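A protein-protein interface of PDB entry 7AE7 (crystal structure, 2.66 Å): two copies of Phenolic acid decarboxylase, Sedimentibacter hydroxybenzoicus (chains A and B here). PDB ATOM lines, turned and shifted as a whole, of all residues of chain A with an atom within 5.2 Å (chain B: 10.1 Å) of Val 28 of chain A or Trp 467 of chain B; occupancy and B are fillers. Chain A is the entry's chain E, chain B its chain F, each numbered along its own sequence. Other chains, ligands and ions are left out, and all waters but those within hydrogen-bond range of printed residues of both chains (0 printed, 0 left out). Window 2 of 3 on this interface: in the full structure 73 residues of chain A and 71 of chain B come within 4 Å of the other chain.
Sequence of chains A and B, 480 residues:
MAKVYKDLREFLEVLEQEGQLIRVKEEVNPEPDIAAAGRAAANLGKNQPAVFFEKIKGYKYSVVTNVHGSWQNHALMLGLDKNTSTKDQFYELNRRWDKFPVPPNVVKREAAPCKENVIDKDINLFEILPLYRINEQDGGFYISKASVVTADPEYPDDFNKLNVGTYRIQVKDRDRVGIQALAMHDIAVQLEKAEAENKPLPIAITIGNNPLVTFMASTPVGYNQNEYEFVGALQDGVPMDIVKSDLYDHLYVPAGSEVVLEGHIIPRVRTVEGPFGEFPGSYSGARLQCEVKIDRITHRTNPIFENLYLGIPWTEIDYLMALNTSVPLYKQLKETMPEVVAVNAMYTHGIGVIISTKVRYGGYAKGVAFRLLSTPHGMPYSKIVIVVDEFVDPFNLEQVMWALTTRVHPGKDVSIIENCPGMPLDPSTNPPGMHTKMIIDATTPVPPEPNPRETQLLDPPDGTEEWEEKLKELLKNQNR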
ATOM      1  N   VAL A  24      16.288   9.964  -5.430  1.00  0.00           N
ATOM      2  CA  VAL A  24      16.570   9.311  -6.703  1.00  0.00           C
ATOM      3  C   VAL A  24      18.049   9.544  -6.990  1.00  0.00           C
ATOM      4  O   VAL A  24      18.434  10.581  -7.537  1.00  0.00           O
ATOM      5  CB  VAL A  24      15.677   9.840  -7.828  1.00  0.00           C
ATOM      6  CG1 VAL A  24      15.897   9.040  -9.105  1.00  0.00           C
ATOM      7  CG2 VAL A  24      14.216   9.792  -7.412  1.00  0.00           C
ATOM      8  N   GLU A  26      20.137   7.820  -8.983  1.00  0.00           N
ATOM      9  CA  GLU A  26      20.504   7.652 -10.381  1.00  0.00           C
ATOM     10  C   GLU A  26      20.234   8.926 -11.176  1.00  0.00           C
ATOM     11  O   GLU A  26      19.385   9.746 -10.814  1.00  0.00           O
ATOM     12  CB  GLU A  26      19.717   6.496 -10.991  1.00  0.00           C
ATOM     13  CG  GLU A  26      18.215   6.734 -10.958  1.00  0.00           C
ATOM     14  CD  GLU A  26      17.408   5.505 -11.314  1.00  0.00           C
ATOM     15  OE1 GLU A  26      17.681   4.429 -10.743  1.00  0.00           O
ATOM     16  OE2 GLU A  26      16.493   5.621 -12.155  1.00  0.00           O
ATOM     17  N   GLU A  27      20.974   9.090 -12.269  1.00  0.00           N
ATOM     18  CA  GLU A  27      20.736  10.208 -13.168  1.00  0.00           C
ATOM     19  C   GLU A  27      19.424  10.016 -13.921  1.00  0.00           C
ATOM     20  O   GLU A  27      19.113   8.917 -14.390  1.00  0.00           O
ATOM     21  CB  GLU A  27      21.891  10.355 -14.157  1.00  0.00           C
ATOM     22  CG  GLU A  27      22.137  11.784 -14.620  1.00  0.00           C
ATOM     23  CD  GLU A  27      23.094  11.863 -15.795  1.00  0.00           C
ATOM     24  OE1 GLU A  27      24.320  11.924 -15.564  1.00  0.00           O
ATOM     25  OE2 GLU A  27      22.619  11.866 -16.951  1.00  0.00           O
ATOM     26  N   VAL A  28      18.654  11.096 -14.038  1.00  0.00           N
ATOM     27  CA  VAL A  28      17.389  11.074 -14.759  1.00  0.00           C
ATOM     28  C   VAL A  28      17.430  12.139 -15.846  1.00  0.00           C
ATOM     29  O   VAL A  28      18.195  13.105 -15.783  1.00  0.00           O
ATOM     30  CB  VAL A  28      16.175  11.296 -13.832  1.00  0.00           C
ATOM     31  CG1 VAL A  28      16.128  10.229 -12.750  1.00  0.00           C
ATOM     32  CG2 VAL A  28      16.216  12.689 -13.218  1.00  0.00           C
ATOM     33  N   ASN A  29      16.598  11.942 -16.861  1.00  0.00           N
ATOM     34  CA  ASN A  29      16.495  12.915 -17.937  1.00  0.00           C
ATOM     35  C   ASN A  29      15.482  13.998 -17.577  1.00  0.00           C
ATOM     36  O   ASN A  29      14.505  13.730 -16.871  1.00  0.00           O
ATOM     37  CB  ASN A  29      16.081  12.227 -19.234  1.00  0.00           C
ATOM     38  CG  ASN A  29      17.202  11.396 -19.831  1.00  0.00           C
ATOM     39  OD1 ASN A  29      16.985  10.274 -20.286  1.00  0.00           O
ATOM     40  ND2 ASN A  29      18.412  11.946 -19.827  1.00  0.00           N
ATOM     41  N   PRO A  30      15.706  15.234 -18.039  1.00  0.00           N
ATOM     42  CA  PRO A  30      14.783  16.326 -17.676  1.00  0.00           C
ATOM     43  C   PRO A  30      13.338  16.047 -18.052  1.00  0.00           C
ATOM     44  O   PRO A  30      12.430  16.306 -17.253  1.00  0.00           O
ATOM     45  CB  PRO A  30      15.349  17.526 -18.448  1.00  0.00           C
ATOM     46  CG  PRO A  30      16.785  17.190 -18.680  1.00  0.00           C
ATOM     47  CD  PRO A  30      16.823  15.705 -18.874  1.00  0.00           C
ATOM     48  N   ASP A  33      10.966  12.528 -17.063  1.00  0.00           N
ATOM     49  CA  ASP A  33      11.175  11.786 -15.823  1.00  0.00           C
ATOM     50  C   ASP A  33      10.766  12.596 -14.599  1.00  0.00           C
ATOM     51  O   ASP A  33      10.090  12.081 -13.704  1.00  0.00           O
ATOM     52  CB  ASP A  33      12.635  11.349 -15.713  1.00  0.00           C
ATOM     53  CG  ASP A  33      13.027  10.352 -16.784  1.00  0.00           C
ATOM     54  OD1 ASP A  33      12.313  10.264 -17.805  1.00  0.00           O
ATOM     55  OD2 ASP A  33      14.046   9.654 -16.600  1.00  0.00           O
ATOM     56  N   ILE A  34      11.170  13.866 -14.534  1.00  0.00           N
ATOM     57  CA  ILE A  34      10.839  14.682 -13.366  1.00  0.00           C
ATOM     58  C   ILE A  34       9.332  14.911 -13.286  1.00  0.00           C
ATOM     59  O   ILE A  34       8.707  14.733 -12.230  1.00  0.00           O
ATOM     60  CB  ILE A  34      11.615  16.011 -13.404  1.00  0.00           C
ATOM     61  CG1 ILE A  34      13.121  15.748 -13.470  1.00  0.00           C
ATOM     62  CG2 ILE A  34      11.278  16.854 -12.189  1.00  0.00           C
ATOM     63  CD1 ILE A  34      13.965  17.010 -13.492  1.00  0.00           C
ATOM     64  N   ALA A  36       6.917  13.138 -14.808  1.00  0.00           N
ATOM     65  CA  ALA A  36       6.231  11.869 -14.600  1.00  0.00           C
ATOM     66  C   ALA A  36       6.386  11.379 -13.169  1.00  0.00           C
ATOM     67  O   ALA A  36       5.473  10.749 -12.632  1.00  0.00           O
ATOM     68  CB  ALA A  36       6.747  10.816 -15.581  1.00  0.00           C
ATOM     69  N   ALA A  37       7.523  11.662 -12.532  1.00  0.00           N
ATOM     70  CA  ALA A  37       7.705  11.263 -11.143  1.00  0.00           C
ATOM     71  C   ALA A  37       6.856  12.113 -10.209  1.00  0.00           C
ATOM     72  O   ALA A  37       6.336  11.606  -9.211  1.00  0.00           O
ATOM     73  CB  ALA A  37       9.180  11.341 -10.760  1.00  0.00           C
ATOM     74  N   ALA A  40       3.498  10.510 -10.607  1.00  0.00           N
ATOM     75  CA  ALA A  40       3.445   9.218  -9.928  1.00  0.00           C
ATOM     76  C   ALA A  40       3.351   9.386  -8.416  1.00  0.00           C
ATOM     77  O   ALA A  40       2.531   8.736  -7.747  1.00  0.00           O
ATOM     78  CB  ALA A  40       4.682   8.399 -10.295  1.00  0.00           C
ATOM     79  N   PHE A  53      15.509  14.483  -6.762  1.00  0.00           N
ATOM     80  CA  PHE A  53      16.417  14.035  -7.809  1.00  0.00           C
ATOM     81  C   PHE A  53      17.781  14.673  -7.588  1.00  0.00           C
ATOM     82  O   PHE A  53      17.902  15.905  -7.594  1.00  0.00           O
ATOM     83  CB  PHE A  53      15.889  14.422  -9.187  1.00  0.00           C
ATOM     84  CG  PHE A  53      14.516  13.921  -9.471  1.00  0.00           C
ATOM     85  CD1 PHE A  53      14.329  12.688 -10.068  1.00  0.00           C
ATOM     86  CD2 PHE A  53      13.408  14.685  -9.148  1.00  0.00           C
ATOM     87  CE1 PHE A  53      13.062  12.226 -10.337  1.00  0.00           C
ATOM     88  CE2 PHE A  53      12.140  14.228  -9.413  1.00  0.00           C
ATOM     89  CZ  PHE A  53      11.968  12.999 -10.009  1.00  0.00           C
ATOM     90  N   LYS A  55      20.560  13.995  -9.581  1.00  0.00           N
ATOM     91  CA  LYS A  55      21.304  14.162 -10.824  1.00  0.00           C
ATOM     92  C   LYS A  55      20.338  14.198 -11.998  1.00  0.00           C
ATOM     93  O   LYS A  55      19.610  13.229 -12.236  1.00  0.00           O
ATOM     94  CB  LYS A  55      22.327  13.037 -11.010  1.00  0.00           C
ATOM     95  N   ILE A  56      20.341  15.309 -12.731  1.00  0.00           N
ATOM     96  CA  ILE A  56      19.555  15.473 -13.949  1.00  0.00           C
ATOM     97  C   ILE A  56      20.524  15.703 -15.100  1.00  0.00           C
ATOM     98  O   ILE A  56      21.434  16.535 -14.991  1.00  0.00           O
ATOM     99  CB  ILE A  56      18.552  16.635 -13.836  1.00  0.00           C
ATOM    100  CG1 ILE A  56      17.707  16.497 -12.567  1.00  0.00           C
ATOM    101  CG2 ILE A  56      17.656  16.684 -15.064  1.00  0.00           C
ATOM    102  CD1 ILE A  56      18.138  17.409 -11.436  1.00  0.00           C
ATOM    103  N   LYS A  57      20.330  14.967 -16.193  1.00  0.00           N
ATOM    104  CA  LYS A  57      21.280  14.972 -17.301  1.00  0.00           C
ATOM    105  C   LYS A  57      21.509  16.382 -17.829  1.00  0.00           C
ATOM    106  O   LYS A  57      20.562  17.102 -18.158  1.00  0.00           O
ATOM    107  CB  LYS A  57      20.772  14.064 -18.424  1.00  0.00           C
ATOM    108  N   PRO B 461       2.044  12.534 -17.921  1.00  0.00           N
ATOM    109  CA  PRO B 461       3.233  12.395 -18.764  1.00  0.00           C
ATOM    110  C   PRO B 461       3.558  10.935 -19.036  1.00  0.00           C
ATOM    111  O   PRO B 461       3.089  10.021 -18.353  1.00  0.00           O
ATOM    112  CB  PRO B 461       4.343  13.062 -17.944  1.00  0.00           C
ATOM    113  CG  PRO B 461       3.644  13.828 -16.859  1.00  0.00           C
ATOM    114  CD  PRO B 461       2.352  13.129 -16.610  1.00  0.00           C
ATOM    115  N   ASP B 462       4.377  10.730 -20.064  1.00  0.00           N
ATOM    116  CA  ASP B 462       4.832   9.389 -20.402  1.00  0.00           C
ATOM    117  C   ASP B 462       5.703   8.823 -19.286  1.00  0.00           C
ATOM    118  O   ASP B 462       6.387   9.556 -18.567  1.00  0.00           O
ATOM    119  CB  ASP B 462       5.614   9.406 -21.715  1.00  0.00           C
ATOM    120  CG  ASP B 462       4.787   8.933 -22.894  1.00  0.00           C
ATOM    121  OD1 ASP B 462       4.352   7.762 -22.883  1.00  0.00           O
ATOM    122  OD2 ASP B 462       4.575   9.731 -23.831  1.00  0.00           O
ATOM    123  N   GLY B 463       5.670   7.502 -19.145  1.00  0.00           N
ATOM    124  CA  GLY B 463       6.446   6.840 -18.120  1.00  0.00           C
ATOM    125  C   GLY B 463       5.897   6.963 -16.719  1.00  0.00           C
ATOM    126  O   GLY B 463       6.613   6.647 -15.762  1.00  0.00           O
ATOM    127  N   THR B 464       4.652   7.418 -16.563  1.00  0.00           N
ATOM    128  CA  THR B 464       4.089   7.599 -15.228  1.00  0.00           C
ATOM    129  C   THR B 464       3.964   6.270 -14.491  1.00  0.00           C
ATOM    130  O   THR B 464       4.312   6.171 -13.311  1.00  0.00           O
ATOM    131  CB  THR B 464       2.731   8.298 -15.322  1.00  0.00           C
ATOM    132  OG1 THR B 464       2.915   9.644 -15.778  1.00  0.00           O
ATOM    133  CG2 THR B 464       2.044   8.317 -13.965  1.00  0.00           C
ATOM    134  N   GLU B 465       3.467   5.233 -15.172  1.00  0.00           N
ATOM    135  CA  GLU B 465       3.284   3.937 -14.520  1.00  0.00           C
ATOM    136  C   GLU B 465       4.620   3.326 -14.104  1.00  0.00           C
ATOM    137  O   GLU B 465       4.761   2.799 -12.986  1.00  0.00           O
ATOM    138  CB  GLU B 465       2.523   2.993 -15.452  1.00  0.00           C
ATOM    139  N   GLU B 466       5.613   3.390 -14.995  1.00  0.00           N
ATOM    140  CA  GLU B 466       6.944   2.899 -14.660  1.00  0.00           C
ATOM    141  C   GLU B 466       7.499   3.627 -13.444  1.00  0.00           C
ATOM    142  O   GLU B 466       8.101   3.007 -12.559  1.00  0.00           O
ATOM    143  CB  GLU B 466       7.875   3.057 -15.863  1.00  0.00           C
ATOM    144  N   TRP B 467       7.280   4.942 -13.369  1.00  0.00           N
ATOM    145  CA  TRP B 467       7.763   5.706 -12.225  1.00  0.00           C
ATOM    146  C   TRP B 467       6.987   5.387 -10.954  1.00  0.00           C
ATOM    147  O   TRP B 467       7.555   5.448  -9.860  1.00  0.00           O
ATOM    148  CB  TRP B 467       7.712   7.200 -12.533  1.00  0.00           C
ATOM    149  CG  TRP B 467       8.975   7.682 -13.159  1.00  0.00           C
ATOM    150  CD1 TRP B 467       9.189   7.952 -14.479  1.00  0.00           C
ATOM    151  CD2 TRP B 467      10.219   7.915 -12.493  1.00  0.00           C
ATOM    152  NE1 TRP B 467      10.488   8.356 -14.674  1.00  0.00           N
ATOM    153  CE2 TRP B 467      11.142   8.341 -13.470  1.00  0.00           C
ATOM    154  CE3 TRP B 467      10.642   7.813 -11.164  1.00  0.00           C
ATOM    155  CZ2 TRP B 467      12.461   8.664 -13.159  1.00  0.00           C
ATOM    156  CZ3 TRP B 467      11.950   8.134 -10.857  1.00  0.00           C
ATOM    157  CH2 TRP B 467      12.845   8.554 -11.850  1.00  0.00           C
ATOM    158  N   GLU B 468       5.699   5.056 -11.067  1.00  0.00           N
ATOM    159  CA  GLU B 468       4.952   4.604  -9.897  1.00  0.00           C
ATOM    160  C   GLU B 468       5.587   3.348  -9.317  1.00  0.00           C
ATOM    161  O   GLU B 468       5.864   3.269  -8.109  1.00  0.00           O
ATOM    162  CB  GLU B 468       3.487   4.353 -10.271  1.00  0.00           C
ATOM    163  CG  GLU B 468       2.729   5.608 -10.689  1.00  0.00           C
ATOM    164  CD  GLU B 468       1.260   5.365 -10.981  1.00  0.00           C
ATOM    165  OE1 GLU B 468       0.667   4.461 -10.359  1.00  0.00           O
ATOM    166  OE2 GLU B 468       0.699   6.086 -11.835  1.00  0.00           O
ATOM    167  N   GLU B 469       5.876   2.371 -10.181  1.00  0.00           N
ATOM    168  CA  GLU B 469       6.549   1.162  -9.712  1.00  0.00           C
ATOM    169  C   GLU B 469       7.923   1.485  -9.121  1.00  0.00           C
ATOM    170  O   GLU B 469       8.298   0.950  -8.066  1.00  0.00           O
ATOM    171  CB  GLU B 469       6.670   0.149 -10.853  1.00  0.00           C
ATOM    172  N   LYS B 470       8.681   2.369  -9.779  1.00  0.00           N
ATOM    173  CA  LYS B 470      10.020   2.712  -9.305  1.00  0.00           C
ATOM    174  C   LYS B 470       9.978   3.347  -7.919  1.00  0.00           C
ATOM    175  O   LYS B 470      10.745   2.970  -7.025  1.00  0.00           O
ATOM    176  CB  LYS B 470      10.705   3.653 -10.298  1.00  0.00           C
ATOM    177  N   LEU B 471       9.094   4.331  -7.730  1.00  0.00           N
ATOM    178  CA  LEU B 471       8.994   5.000  -6.439  1.00  0.00           C
ATOM    179  C   LEU B 471       8.529   4.040  -5.356  1.00  0.00           C
ATOM    180  O   LEU B 471       8.977   4.134  -4.207  1.00  0.00           O
ATOM    181  CB  LEU B 471       8.052   6.201  -6.524  1.00  0.00           C
ATOM    182  CG  LEU B 471       8.465   7.376  -7.409  1.00  0.00           C
ATOM    183  CD1 LEU B 471       7.457   8.510  -7.277  1.00  0.00           C
ATOM    184  CD2 LEU B 471       9.865   7.851  -7.057  1.00  0.00           C
ATOM    185  N   LYS B 472       7.624   3.115  -5.690  1.00  0.00           N
ATOM    186  CA  LYS B 472       7.228   2.118  -4.698  1.00  0.00           C
ATOM    187  C   LYS B 472       8.415   1.258  -4.279  1.00  0.00           C
ATOM    188  O   LYS B 472       8.595   0.969  -3.087  1.00  0.00           O
ATOM    189  CB  LYS B 472       6.095   1.252  -5.242  1.00  0.00           C
ATOM    190  CG  LYS B 472       4.737   1.918  -5.173  1.00  0.00           C
ATOM    191  CD  LYS B 472       3.631   0.904  -5.367  1.00  0.00           C
ATOM    192  CE  LYS B 472       2.697   1.325  -6.483  1.00  0.00           C
ATOM    193  NZ  LYS B 472       1.890   0.180  -6.988  1.00  0.00           N
ATOM    194  N   GLU B 473       9.242   0.847  -5.246  1.00  0.00           N
ATOM    195  CA  GLU B 473      10.425   0.058  -4.910  1.00  0.00           C
ATOM    196  C   GLU B 473      11.397   0.854  -4.047  1.00  0.00           C
ATOM    197  O   GLU B 473      12.015   0.308  -3.126  1.00  0.00           O
ATOM    198  CB  GLU B 473      11.115  -0.428  -6.185  1.00  0.00           C
ATOM    199  N   LEU B 474      11.551   2.148  -4.337  1.00  0.00           N
ATOM    200  CA  LEU B 474      12.447   2.982  -3.538  1.00  0.00           C
ATOM    201  C   LEU B 474      11.903   3.214  -2.133  1.00  0.00           C
ATOM    202  O   LEU B 474      12.682   3.347  -1.182  1.00  0.00           O
ATOM    203  CB  LEU B 474      12.695   4.317  -4.241  1.00  0.00           C
ATOM    204  CG  LEU B 474      13.915   4.373  -5.165  1.00  0.00           C
ATOM    205  CD1 LEU B 474      13.724   3.492  -6.390  1.00  0.00           C
ATOM    206  CD2 LEU B 474      14.213   5.809  -5.575  1.00  0.00           C
ATOM    207  N   LEU B 475      10.577   3.274  -1.987  1.00  0.00           N
ATOM    208  CA  LEU B 475       9.969   3.417  -0.668  1.00  0.00           C
ATOM    209  C   LEU B 475      10.091   2.139   0.150  1.00  0.00           C
ATOM    210  O   LEU B 475      10.239   2.203   1.377  1.00  0.00           O
ATOM    211  CB  LEU B 475       8.499   3.809  -0.808  1.00  0.00           C
ATOM    212  CG  LEU B 475       8.176   5.292  -0.622  1.00  0.00           C
ATOM    213  CD1 LEU B 475       6.738   5.583  -1.022  1.00  0.00           C
ATOM    214  CD2 LEU B 475       8.437   5.734   0.810  1.00  0.00           C
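O of Val 28 of chain A is in hydrogen-bond range of N of Lys 57 of chain A. N of Asn 29 of chain A lies within hydrogen-bond range of OD2 of Asp 33 of chain A, 3.4 Å away. The side-chain hydroxyl of Thr 464 of chain B lies within hydrogen-bond range of the backbone carbonyl oxygen of Pro 461 of chain B (2.6 Å). The backbone NH (N) of Val 28 of chain A sits at hydrogen-bond distance from the backbone carbonyl oxygen (O) of Lys 55 of chain A.
No position is printed for both chains. Of the 11 pairs that touch across the chains among the printed residues, none has its exchanged pair printed and touching as well.
Printed residues of chain B within 4 Å of Val 28 of chain A: Trp 467 (3.8 Å). Of chain A, only Val 28, Asp 33, Ala 36, Ala 37, Ala 40 and Phe 53 come within 4 Å of Trp 467 of chain B. No residue of chain B comes within 4 Å of Glu 27 of chain A. No residue of chain B comes within 4 Å of Asn 29 of chain A. Asp 33 of chain A touches one residue of chain B. No residue of chain B comes within 4 Å of Lys 55 of chain A. No residue of chain B comes within 4 Å of Lys 57 of chain A. Of the printed residues of chain A, Leu 471 of chain B touches Ala 37. Of the printed residues of chain B, Ala 40 of chain A touches Thr 464, Trp 467 and Glu 468. Of the printed residues of chain A, Pro 461 of chain B touches Ala 36 (3.9 Å). Of the printed residues of chain B, Ala 36 of chain A touches Pro 461, Asp 462 and Trp 467. Of the printed residues of chain A, Asp 462 of chain B touches Ala 36 (3.3 Å). Glu 473 of chain B touches none of the printed residues of chain A. Gly 463 of chain B touches none of the printed residues of chain A. The nearest residue of chain B that does not touch Val 28 of chain A is Leu 474 of chain B (8.6 Å). The nearest residue of chain A that does not touch Trp 467 of chain B is Val 24 of chain A (4.1 Å).
Of the 15 printed residues of chain B, 6 touch a printed residue of chain A. Printed residues of chain B that touch a printed residue of chain A: Pro 461, Asp 462, Thr 464, Trp 467, Glu 468 and Leu 471. Hydrophobic or aromatic side chains of chain A that line the printed part of chain B: Val 28, Ala 36, Ala 37, Ala 40 and Phe 53.
Among the printed residues, pairs that only touch across the chains: Val 28 of chain A with Trp 467 of chain B, Asp 33 of chain A with Trp 467 of chain B, Ala 36 of chain A with Pro 461 of chain B, Ala 36 of chain A with Asp 462 of chain B, Ala 36 of chain A with Trp 467 of chain B, Ala 37 of chain A with Trp 467 of chain B, Ala 37 of chain A with Leu 471 of chain B, Ala 40 of chain A with Thr 464 of chain B, Ala 40 of chain A with Trp 467 of chain B, Ala 40 of chain A with Glu 468 of chain B and Phe 53 of chain A with Trp 467 of chain B.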
